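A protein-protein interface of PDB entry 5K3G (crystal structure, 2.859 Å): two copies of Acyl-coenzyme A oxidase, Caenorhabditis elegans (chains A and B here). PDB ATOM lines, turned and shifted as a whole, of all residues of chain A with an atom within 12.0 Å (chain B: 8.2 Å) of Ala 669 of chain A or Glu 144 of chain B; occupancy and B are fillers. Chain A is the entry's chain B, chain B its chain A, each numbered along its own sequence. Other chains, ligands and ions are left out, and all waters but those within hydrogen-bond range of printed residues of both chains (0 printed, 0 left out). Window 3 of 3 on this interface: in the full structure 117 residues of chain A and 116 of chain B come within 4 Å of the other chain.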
ATOM      1  N   VAL A 658     -14.652  21.098  -4.120  1.00  0.00           N
ATOM      2  CA  VAL A 658     -13.608  22.118  -4.079  1.00  0.00           C
ATOM      3  C   VAL A 658     -12.352  21.590  -3.397  1.00  0.00           C
ATOM      4  O   VAL A 658     -11.234  22.001  -3.725  1.00  0.00           O
ATOM      5  CB  VAL A 658     -14.127  23.386  -3.375  1.00  0.00           C
ATOM      6  CG1 VAL A 658     -13.009  24.423  -3.229  1.00  0.00           C
ATOM      7  CG2 VAL A 658     -15.300  23.977  -4.133  1.00  0.00           C
ATOM      8  N   TYR A 661     -11.161  18.286  -6.052  1.00  0.00           N
ATOM      9  CA  TYR A 661     -10.939  18.907  -7.352  1.00  0.00           C
ATOM     10  C   TYR A 661     -11.036  20.420  -7.181  1.00  0.00           C
ATOM     11  O   TYR A 661     -11.189  20.917  -6.066  1.00  0.00           O
ATOM     12  CB  TYR A 661     -11.959  18.388  -8.374  1.00  0.00           C
ATOM     13  CG  TYR A 661     -12.141  16.875  -8.385  1.00  0.00           C
ATOM     14  CD1 TYR A 661     -11.224  16.047  -9.023  1.00  0.00           C
ATOM     15  CD2 TYR A 661     -13.236  16.280  -7.766  1.00  0.00           C
ATOM     16  CE1 TYR A 661     -11.385  14.663  -9.035  1.00  0.00           C
ATOM     17  CE2 TYR A 661     -13.408  14.896  -7.779  1.00  0.00           C
ATOM     18  CZ  TYR A 661     -12.478  14.093  -8.410  1.00  0.00           C
ATOM     19  OH  TYR A 661     -12.644  12.720  -8.418  1.00  0.00           O
ATOM     20  N   LEU A 662     -10.964  21.152  -8.293  1.00  0.00           N
ATOM     21  CA  LEU A 662     -11.208  22.592  -8.311  1.00  0.00           C
ATOM     22  C   LEU A 662     -10.119  23.375  -7.580  1.00  0.00           C
ATOM     23  O   LEU A 662      -9.480  24.234  -8.199  1.00  0.00           O
ATOM     24  CB  LEU A 662     -12.586  22.937  -7.738  1.00  0.00           C
ATOM     25  CG  LEU A 662     -13.731  23.072  -8.762  1.00  0.00           C
ATOM     26  CD1 LEU A 662     -13.616  22.060  -9.919  1.00  0.00           C
ATOM     27  CD2 LEU A 662     -15.081  22.927  -8.074  1.00  0.00           C
ATOM     28  N   LYS A 663      -9.876  23.116  -6.281  1.00  0.00           N
ATOM     29  CA  LYS A 663      -8.805  23.908  -5.663  1.00  0.00           C
ATOM     30  C   LYS A 663      -7.427  23.374  -6.055  1.00  0.00           C
ATOM     31  O   LYS A 663      -6.511  24.172  -6.295  1.00  0.00           O
ATOM     32  CB  LYS A 663      -8.923  23.993  -4.136  1.00  0.00           C
ATOM     33  CG  LYS A 663      -8.227  25.235  -3.576  1.00  0.00           C
ATOM     34  CD  LYS A 663      -7.977  25.216  -2.069  1.00  0.00           C
ATOM     35  CE  LYS A 663      -9.003  24.406  -1.309  1.00  0.00           C
ATOM     36  NZ  LYS A 663      -8.634  24.311   0.132  1.00  0.00           N
ATOM     37  N   PRO A 664      -7.217  22.055  -6.121  1.00  0.00           N
ATOM     38  CA  PRO A 664      -5.987  21.569  -6.771  1.00  0.00           C
ATOM     39  C   PRO A 664      -5.841  22.054  -8.201  1.00  0.00           C
ATOM     40  O   PRO A 664      -4.714  22.255  -8.673  1.00  0.00           O
ATOM     41  CB  PRO A 664      -6.143  20.046  -6.700  1.00  0.00           C
ATOM     42  CG  PRO A 664      -6.911  19.828  -5.454  1.00  0.00           C
ATOM     43  CD  PRO A 664      -7.897  20.969  -5.381  1.00  0.00           C
ATOM     44  N   MET A 665      -6.961  22.254  -8.902  1.00  0.00           N
ATOM     45  CA  MET A 665      -6.917  22.784 -10.259  1.00  0.00           C
ATOM     46  C   MET A 665      -6.436  24.229 -10.277  1.00  0.00           C
ATOM     47  O   MET A 665      -5.597  24.598 -11.107  1.00  0.00           O
ATOM     48  CB  MET A 665      -8.299  22.678 -10.895  1.00  0.00           C
ATOM     49  CG  MET A 665      -8.349  23.151 -12.326  1.00  0.00           C
ATOM     50  SD  MET A 665     -10.036  23.424 -12.883  1.00  0.00           S
ATOM     51  CE  MET A 665     -10.469  24.881 -11.937  1.00  0.00           C
ATOM     52  N   MET A 666      -6.961  25.063  -9.373  1.00  0.00           N
ATOM     53  CA  MET A 666      -6.551  26.464  -9.338  1.00  0.00           C
ATOM     54  C   MET A 666      -5.109  26.607  -8.876  1.00  0.00           C
ATOM     55  O   MET A 666      -4.365  27.444  -9.401  1.00  0.00           O
ATOM     56  CB  MET A 666      -7.482  27.269  -8.433  1.00  0.00           C
ATOM     57  CG  MET A 666      -8.883  27.437  -8.986  1.00  0.00           C
ATOM     58  SD  MET A 666      -9.929  28.497  -7.972  1.00  0.00           S
ATOM     59  CE  MET A 666     -10.015  27.545  -6.458  1.00  0.00           C
ATOM     60  N   GLU A 667      -4.699  25.805  -7.891  1.00  0.00           N
ATOM     61  CA  GLU A 667      -3.312  25.847  -7.439  1.00  0.00           C
ATOM     62  C   GLU A 667      -2.359  25.493  -8.572  1.00  0.00           C
ATOM     63  O   GLU A 667      -1.328  26.151  -8.757  1.00  0.00           O
ATOM     64  CB  GLU A 667      -3.120  24.915  -6.240  1.00  0.00           C
ATOM     65  CG  GLU A 667      -3.155  25.656  -4.911  1.00  0.00           C
ATOM     66  CD  GLU A 667      -3.860  24.884  -3.811  1.00  0.00           C
ATOM     67  OE1 GLU A 667      -4.153  25.488  -2.757  1.00  0.00           O
ATOM     68  OE2 GLU A 667      -4.122  23.677  -3.991  1.00  0.00           O
ATOM     69  N   LYS A 668      -2.701  24.474  -9.365  1.00  0.00           N
ATOM     70  CA  LYS A 668      -1.802  24.041 -10.432  1.00  0.00           C
ATOM     71  C   LYS A 668      -1.647  25.122 -11.494  1.00  0.00           C
ATOM     72  O   LYS A 668      -0.551  25.341 -12.021  1.00  0.00           O
ATOM     73  CB  LYS A 668      -2.309  22.740 -11.061  1.00  0.00           C
ATOM     74  CG  LYS A 668      -1.257  22.046 -11.924  1.00  0.00           C
ATOM     75  CD  LYS A 668      -1.711  20.706 -12.497  1.00  0.00           C
ATOM     76  CE  LYS A 668      -0.645  20.166 -13.443  1.00  0.00           C
ATOM     77  NZ  LYS A 668      -0.805  18.734 -13.816  1.00  0.00           N
ATOM     78  N   ALA A 669      -2.735  25.818 -11.805  1.00  0.00           N
ATOM     79  CA  ALA A 669      -2.759  26.797 -12.881  1.00  0.00           C
ATOM     80  C   ALA A 669      -1.768  27.928 -12.644  1.00  0.00           C
ATOM     81  O   ALA A 669      -1.496  28.297 -11.504  1.00  0.00           O
ATOM     82  CB  ALA A 669      -4.162  27.351 -13.048  1.00  0.00           C
ATOM     83  N   THR B  83     -10.059  20.462 -18.605  1.00  0.00           N
ATOM     84  CA  THR B  83      -9.063  21.529 -18.715  1.00  0.00           C
ATOM     85  C   THR B  83      -7.717  21.001 -19.199  1.00  0.00           C
ATOM     86  O   THR B  83      -6.956  21.736 -19.837  1.00  0.00           O
ATOM     87  CB  THR B  83      -8.863  22.257 -17.381  1.00  0.00           C
ATOM     88  OG1 THR B  83      -7.867  21.583 -16.597  1.00  0.00           O
ATOM     89  CG2 THR B  83     -10.146  22.332 -16.596  1.00  0.00           C
ATOM     90  N   MET B 113     -18.546  25.424 -13.207  1.00  0.00           N
ATOM     91  CA  MET B 113     -18.017  26.602 -13.885  1.00  0.00           C
ATOM     92  C   MET B 113     -18.913  27.047 -15.034  1.00  0.00           C
ATOM     93  O   MET B 113     -18.433  27.673 -15.984  1.00  0.00           O
ATOM     94  CB  MET B 113     -16.589  26.346 -14.370  1.00  0.00           C
ATOM     95  CG  MET B 113     -15.592  26.191 -13.224  1.00  0.00           C
ATOM     96  SD  MET B 113     -13.939  25.671 -13.718  1.00  0.00           S
ATOM     97  CE  MET B 113     -13.228  27.223 -14.249  1.00  0.00           C
ATOM     98  N   HIS B 116     -18.726  30.725 -15.245  1.00  0.00           N
ATOM     99  CA  HIS B 116     -17.378  31.246 -15.445  1.00  0.00           C
ATOM    100  C   HIS B 116     -17.181  31.694 -16.888  1.00  0.00           C
ATOM    101  O   HIS B 116     -16.682  32.795 -17.144  1.00  0.00           O
ATOM    102  CB  HIS B 116     -16.342  30.189 -15.054  1.00  0.00           C
ATOM    103  CG  HIS B 116     -14.922  30.668 -15.111  1.00  0.00           C
ATOM    104  ND1 HIS B 116     -14.360  31.454 -14.129  1.00  0.00           N
ATOM    105  CD2 HIS B 116     -13.944  30.455 -16.023  1.00  0.00           C
ATOM    106  CE1 HIS B 116     -13.102  31.714 -14.438  1.00  0.00           C
ATOM    107  NE2 HIS B 116     -12.825  31.120 -15.584  1.00  0.00           N
ATOM    108  N   LYS B 135      -4.934  41.721 -15.039  1.00  0.00           N
ATOM    109  CA  LYS B 135      -4.771  41.029 -13.765  1.00  0.00           C
ATOM    110  C   LYS B 135      -5.905  40.050 -13.478  1.00  0.00           C
ATOM    111  O   LYS B 135      -5.675  39.015 -12.845  1.00  0.00           O
ATOM    112  CB  LYS B 135      -4.615  42.042 -12.619  1.00  0.00           C
ATOM    113  CG  LYS B 135      -5.877  42.452 -11.879  1.00  0.00           C
ATOM    114  CD  LYS B 135      -5.558  43.526 -10.841  1.00  0.00           C
ATOM    115  CE  LYS B 135      -5.200  44.839 -11.529  1.00  0.00           C
ATOM    116  NZ  LYS B 135      -5.176  46.020 -10.614  1.00  0.00           N
ATOM    117  N   TRP B 136      -7.116  40.321 -13.958  1.00  0.00           N
ATOM    118  CA  TRP B 136      -8.252  39.467 -13.630  1.00  0.00           C
ATOM    119  C   TRP B 136      -8.729  38.596 -14.786  1.00  0.00           C
ATOM    120  O   TRP B 136      -9.066  37.433 -14.561  1.00  0.00           O
ATOM    121  CB  TRP B 136      -9.416  40.317 -13.120  1.00  0.00           C
ATOM    122  CG  TRP B 136      -9.171  40.920 -11.776  1.00  0.00           C
ATOM    123  CD1 TRP B 136      -8.561  40.339 -10.698  1.00  0.00           C
ATOM    124  CD2 TRP B 136      -9.527  42.240 -11.372  1.00  0.00           C
ATOM    125  NE1 TRP B 136      -8.530  41.223  -9.643  1.00  0.00           N
ATOM    126  CE2 TRP B 136      -9.119  42.397 -10.033  1.00  0.00           C
ATOM    127  CE3 TRP B 136     -10.164  43.306 -12.012  1.00  0.00           C
ATOM    128  CZ2 TRP B 136      -9.327  43.578  -9.326  1.00  0.00           C
ATOM    129  CZ3 TRP B 136     -10.369  44.471 -11.316  1.00  0.00           C
ATOM    130  CH2 TRP B 136      -9.951  44.603  -9.987  1.00  0.00           C
ATOM    131  N   LEU B 137      -8.786  39.120 -16.015  1.00  0.00           N
ATOM    132  CA  LEU B 137      -9.295  38.311 -17.123  1.00  0.00           C
ATOM    133  C   LEU B 137      -8.330  37.185 -17.464  1.00  0.00           C
ATOM    134  O   LEU B 137      -8.757  36.072 -17.793  1.00  0.00           O
ATOM    135  CB  LEU B 137      -9.569  39.185 -18.351  1.00  0.00           C
ATOM    136  CG  LEU B 137      -9.950  38.480 -19.663  1.00  0.00           C
ATOM    137  CD1 LEU B 137     -11.177  37.586 -19.488  1.00  0.00           C
ATOM    138  CD2 LEU B 137     -10.186  39.512 -20.756  1.00  0.00           C
ATOM    139  N   ILE B 138      -7.026  37.450 -17.375  1.00  0.00           N
ATOM    140  CA  ILE B 138      -6.030  36.420 -17.667  1.00  0.00           C
ATOM    141  C   ILE B 138      -6.155  35.266 -16.685  1.00  0.00           C
ATOM    142  O   ILE B 138      -6.088  34.090 -17.064  1.00  0.00           O
ATOM    143  CB  ILE B 138      -4.611  37.020 -17.655  1.00  0.00           C
ATOM    144  CG1 ILE B 138      -4.473  38.034 -18.785  1.00  0.00           C
ATOM    145  CG2 ILE B 138      -3.560  35.920 -17.752  1.00  0.00           C
ATOM    146  CD1 ILE B 138      -4.784  37.452 -20.144  1.00  0.00           C
ATOM    147  N   ARG B 139      -6.338  35.587 -15.403  1.00  0.00           N
ATOM    148  CA  ARG B 139      -6.485  34.544 -14.393  1.00  0.00           C
ATOM    149  C   ARG B 139      -7.744  33.723 -14.631  1.00  0.00           C
ATOM    150  O   ARG B 139      -7.740  32.500 -14.445  1.00  0.00           O
ATOM    151  CB  ARG B 139      -6.508  35.163 -12.995  1.00  0.00           C
ATOM    152  CG  ARG B 139      -5.243  35.935 -12.639  1.00  0.00           C
ATOM    153  CD  ARG B 139      -5.200  36.253 -11.154  1.00  0.00           C
ATOM    154  NE  ARG B 139      -4.981  35.062 -10.336  1.00  0.00           N
ATOM    155  CZ  ARG B 139      -5.301  34.975  -9.048  1.00  0.00           C
ATOM    156  NH1 ARG B 139      -5.866  36.008  -8.436  1.00  0.00           N
ATOM    157  NH2 ARG B 139      -5.069  33.855  -8.377  1.00  0.00           N
ATOM    158  N   ALA B 140      -8.836  34.380 -15.025  1.00  0.00           N
ATOM    159  CA  ALA B 140     -10.068  33.663 -15.336  1.00  0.00           C
ATOM    160  C   ALA B 140      -9.859  32.715 -16.508  1.00  0.00           C
ATOM    161  O   ALA B 140     -10.185  31.525 -16.424  1.00  0.00           O
ATOM    162  CB  ALA B 140     -11.196  34.654 -15.639  1.00  0.00           C
ATOM    163  N   LEU B 141      -9.280  33.224 -17.603  1.00  0.00           N
ATOM    164  CA  LEU B 141      -9.041  32.394 -18.782  1.00  0.00           C
ATOM    165  C   LEU B 141      -8.196  31.176 -18.441  1.00  0.00           C
ATOM    166  O   LEU B 141      -8.400  30.091 -18.998  1.00  0.00           O
ATOM    167  CB  LEU B 141      -8.364  33.213 -19.882  1.00  0.00           C
ATOM    168  CG  LEU B 141      -9.233  34.248 -20.600  1.00  0.00           C
ATOM    169  CD1 LEU B 141      -8.397  35.159 -21.481  1.00  0.00           C
ATOM    170  CD2 LEU B 141     -10.274  33.520 -21.421  1.00  0.00           C
ATOM    171  N   ARG B 142      -7.245  31.335 -17.526  1.00  0.00           N
ATOM    172  CA  ARG B 142      -6.350  30.254 -17.143  1.00  0.00           C
ATOM    173  C   ARG B 142      -6.906  29.399 -16.016  1.00  0.00           C
ATOM    174  O   ARG B 142      -6.216  28.484 -15.555  1.00  0.00           O
ATOM    175  CB  ARG B 142      -4.995  30.835 -16.756  1.00  0.00           C
ATOM    176  CG  ARG B 142      -4.280  31.495 -17.917  1.00  0.00           C
ATOM    177  CD  ARG B 142      -3.125  32.349 -17.430  1.00  0.00           C
ATOM    178  NE  ARG B 142      -2.381  31.705 -16.350  1.00  0.00           N
ATOM    179  CZ  ARG B 142      -1.455  30.770 -16.538  1.00  0.00           C
ATOM    180  NH1 ARG B 142      -1.161  30.361 -17.763  1.00  0.00           N
ATOM    181  NH2 ARG B 142      -0.824  30.237 -15.500  1.00  0.00           N
ATOM    182  N   ARG B 143      -8.130  29.681 -15.570  1.00  0.00           N
ATOM    183  CA  ARG B 143      -8.814  28.879 -14.561  1.00  0.00           C
ATOM    184  C   ARG B 143      -8.019  28.829 -13.253  1.00  0.00           C
ATOM    185  O   ARG B 143      -8.048  27.830 -12.529  1.00  0.00           O
ATOM    186  CB  ARG B 143      -9.128  27.481 -15.118  1.00  0.00           C
ATOM    187  CG  ARG B 143     -10.072  27.558 -16.352  1.00  0.00           C
ATOM    188  CD  ARG B 143     -10.422  26.209 -17.017  1.00  0.00           C
ATOM    189  NE  ARG B 143     -11.767  26.253 -17.603  1.00  0.00           N
ATOM    190  CZ  ARG B 143     -12.305  25.317 -18.384  1.00  0.00           C
ATOM    191  NH1 ARG B 143     -11.623  24.230 -18.707  1.00  0.00           N
ATOM    192  NH2 ARG B 143     -13.539  25.475 -18.850  1.00  0.00           N
ATOM    193  N   GLU B 144      -7.302  29.924 -12.958  1.00  0.00           N
ATOM    194  CA  GLU B 144      -6.720  30.167 -11.641  1.00  0.00           C
ATOM    195  C   GLU B 144      -7.753  30.625 -10.624  1.00  0.00           C
ATOM    196  O   GLU B 144      -7.529  30.472  -9.418  1.00  0.00           O
ATOM    197  CB  GLU B 144      -5.635  31.245 -11.707  1.00  0.00           C
ATOM    198  CG  GLU B 144      -4.384  30.910 -12.493  1.00  0.00           C
ATOM    199  CD  GLU B 144      -3.403  32.073 -12.504  1.00  0.00           C
ATOM    200  OE1 GLU B 144      -3.615  33.024 -11.722  1.00  0.00           O
ATOM    201  OE2 GLU B 144      -2.434  32.047 -13.295  1.00  0.00           O
ATOM    202  N   ILE B 145      -8.845  31.234 -11.081  1.00  0.00           N
ATOM    203  CA  ILE B 145      -9.952  31.632 -10.226  1.00  0.00           C
ATOM    204  C   ILE B 145     -11.235  31.112 -10.860  1.00  0.00           C
ATOM    205  O   ILE B 145     -11.297  30.836 -12.061  1.00  0.00           O
ATOM    206  CB  ILE B 145     -10.035  33.163 -10.033  1.00  0.00           C
ATOM    207  CG1 ILE B 145     -10.155  33.850 -11.393  1.00  0.00           C
ATOM    208  CG2 ILE B 145      -8.823  33.690  -9.265  1.00  0.00           C
ATOM    209  CD1 ILE B 145     -10.480  35.322 -11.324  1.00  0.00           C
ATOM    210  N   ILE B 146     -12.261  30.961 -10.031  1.00  0.00           N
ATOM    211  CA  ILE B 146     -13.601  30.617 -10.485  1.00  0.00           C
ATOM    212  C   ILE B 146     -14.511  31.774 -10.110  1.00  0.00           C
ATOM    213  O   ILE B 146     -14.491  32.237  -8.964  1.00  0.00           O
ATOM    214  CB  ILE B 146     -14.095  29.294  -9.871  1.00  0.00           C
ATOM    215  CG1 ILE B 146     -13.131  28.158 -10.220  1.00  0.00           C
ATOM    216  CG2 ILE B 146     -15.504  28.955 -10.361  1.00  0.00           C
ATOM    217  CD1 ILE B 146     -13.445  26.857  -9.504  1.00  0.00           C
ATOM    218  N   GLY B 147     -15.294  32.258 -11.079  1.00  0.00           N
ATOM    219  CA  GLY B 147     -16.076  33.460 -10.884  1.00  0.00           C
ATOM    220  C   GLY B 147     -17.457  33.353 -11.498  1.00  0.00           C
ATOM    221  O   GLY B 147     -17.745  32.451 -12.290  1.00  0.00           O
ATOM    222  N   ASN B 198     -14.819  31.856  -6.135  1.00  0.00           N
ATOM    223  CA  ASN B 198     -14.178  32.702  -5.135  1.00  0.00           C
ATOM    224  C   ASN B 198     -14.120  34.168  -5.553  1.00  0.00           C
ATOM    225  O   ASN B 198     -13.693  35.008  -4.756  1.00  0.00           O
ATOM    226  CB  ASN B 198     -12.772  32.191  -4.785  1.00  0.00           C
ATOM    227  CG  ASN B 198     -11.953  31.821  -6.001  1.00  0.00           C
ATOM    228  OD1 ASN B 198     -12.264  32.201  -7.127  1.00  0.00           O
ATOM    229  ND2 ASN B 198     -10.870  31.088  -5.768  1.00  0.00           N
ATOM    230  N   TYR B 199     -14.563  34.505  -6.765  1.00  0.00           N
ATOM    231  CA  TYR B 199     -14.725  35.892  -7.178  1.00  0.00           C
ATOM    232  C   TYR B 199     -16.081  36.070  -7.844  1.00  0.00           C
ATOM    233  O   TYR B 199     -16.717  35.105  -8.273  1.00  0.00           O
ATOM    234  CB  TYR B 199     -13.619  36.346  -8.139  1.00  0.00           C
ATOM    235  CG  TYR B 199     -12.291  36.608  -7.468  1.00  0.00           C
ATOM    236  CD1 TYR B 199     -11.451  35.560  -7.117  1.00  0.00           C
ATOM    237  CD2 TYR B 199     -11.880  37.904  -7.180  1.00  0.00           C
ATOM    238  CE1 TYR B 199     -10.237  35.797  -6.497  1.00  0.00           C
ATOM    239  CE2 TYR B 199     -10.671  38.148  -6.563  1.00  0.00           C
ATOM    240  CZ  TYR B 199      -9.854  37.091  -6.223  1.00  0.00           C
ATOM    241  OH  TYR B 199      -8.645  37.321  -5.614  1.00  0.00           O
ATOM    242  N   GLU B 225      -8.142  32.677  -1.263  1.00  0.00           N
ATOM    243  CA  GLU B 225      -7.615  31.841  -2.335  1.00  0.00           C
ATOM    244  C   GLU B 225      -6.885  30.611  -1.808  1.00  0.00           C
ATOM    245  O   GLU B 225      -6.664  29.663  -2.571  1.00  0.00           O
ATOM    246  CB  GLU B 225      -6.708  32.663  -3.253  1.00  0.00           C
ATOM    247  CG  GLU B 225      -7.454  33.792  -3.966  1.00  0.00           C
ATOM    248  CD  GLU B 225      -6.738  34.313  -5.196  1.00  0.00           C
ATOM    249  OE1 GLU B 225      -5.928  33.561  -5.778  1.00  0.00           O
ATOM    250  OE2 GLU B 225      -6.996  35.471  -5.590  1.00  0.00           O
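The backbone carbonyl oxygen of Ile 146 of chain B sits at hydrogen-bond distance from the backbone NH of Asn 198 of chain B (2.9 Å).
OE1 of Glu 144 of chain B is in salt-bridge range of NE of Arg 139 of chain B (2.8 Å).
The side-chain carboxylate of Glu 144 of chain B is in salt-bridge range of the guanidinium group of Arg 142 of chain B (3.1 Å).
The backbone carbonyl oxygen of Ile 146 of chain B lies within hydrogen-bond range of the backbone NH of Tyr 199 of chain B (3.2 Å).
Tyr 661 of chain A touches none of the printed residues of chain B.
Of chain B, only Arg 142 (3.4 Å), Arg 143 (3.9 Å) and Glu 144 (3.6 Å) come within 4 Å of Ala 669 of chain A.
Ile 138 of chain B touches none of the printed residues of chain A.
No residue of chain A comes within 4 Å of Arg 139 of chain B.
No residue of chain A comes within 4 Å of Ala 140 of chain B.
Of the printed residues of chain A, Arg 143 of chain B touches Met 665, Met 666 and Ala 669.
Of the printed residues of chain A, Glu 144 of chain B touches Met 666 and Ala 669.
Ile 145 of chain B touches just one residue of chain A: Met 666 (3.9 Å).
Of chain A, only Leu 662 (3.9 Å) and Met 666 (3.9 Å) come within 4 Å of Ile 146 of chain B.
Printed residues of chain A within 4 Å of Asn 198 of chain B: Met 666 (3.5 Å).
No position is printed for both chains.
The side-chain sulfur (SD) of Met 666 of chain A sits close to the backbone carbonyl oxygen (O) of Glu 144 of chain B (3.4 Å).
SD of Met 666 of chain A lies within hydrogen-bond range of ND2 of Asn 198 of chain B (3.5 Å).
Among the printed residues, pairs that only touch across the chains: Leu 662 of chain A with Ile 146 of chain B (3.9 Å), Met 665 of chain A with Thr 83 of chain B (3.9 Å), Met 665 of chain A with Met 113 of chain B (3.98 Å), Met 665 of chain A with Arg 143 of chain B (3.9 Å), Met 666 of chain A with Arg 143 of chain B (3.7 Å), Met 666 of chain A with Ile 145 of chain B (3.9 Å), Met 666 of chain A with Ile 146 of chain B (3.9 Å), Ala 669 of chain A with Arg 142 of chain B (3.4 Å), Ala 669 of chain A with Arg 143 of chain B (3.9 Å) and Ala 669 of chain A with Glu 144 of chain B (3.6 Å).
Of the 10 printed residues of chain A, 4 touch a printed residue of chain B.
Along chain A the printed residues that touch a printed residue of chain B span positions 662 to 669.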
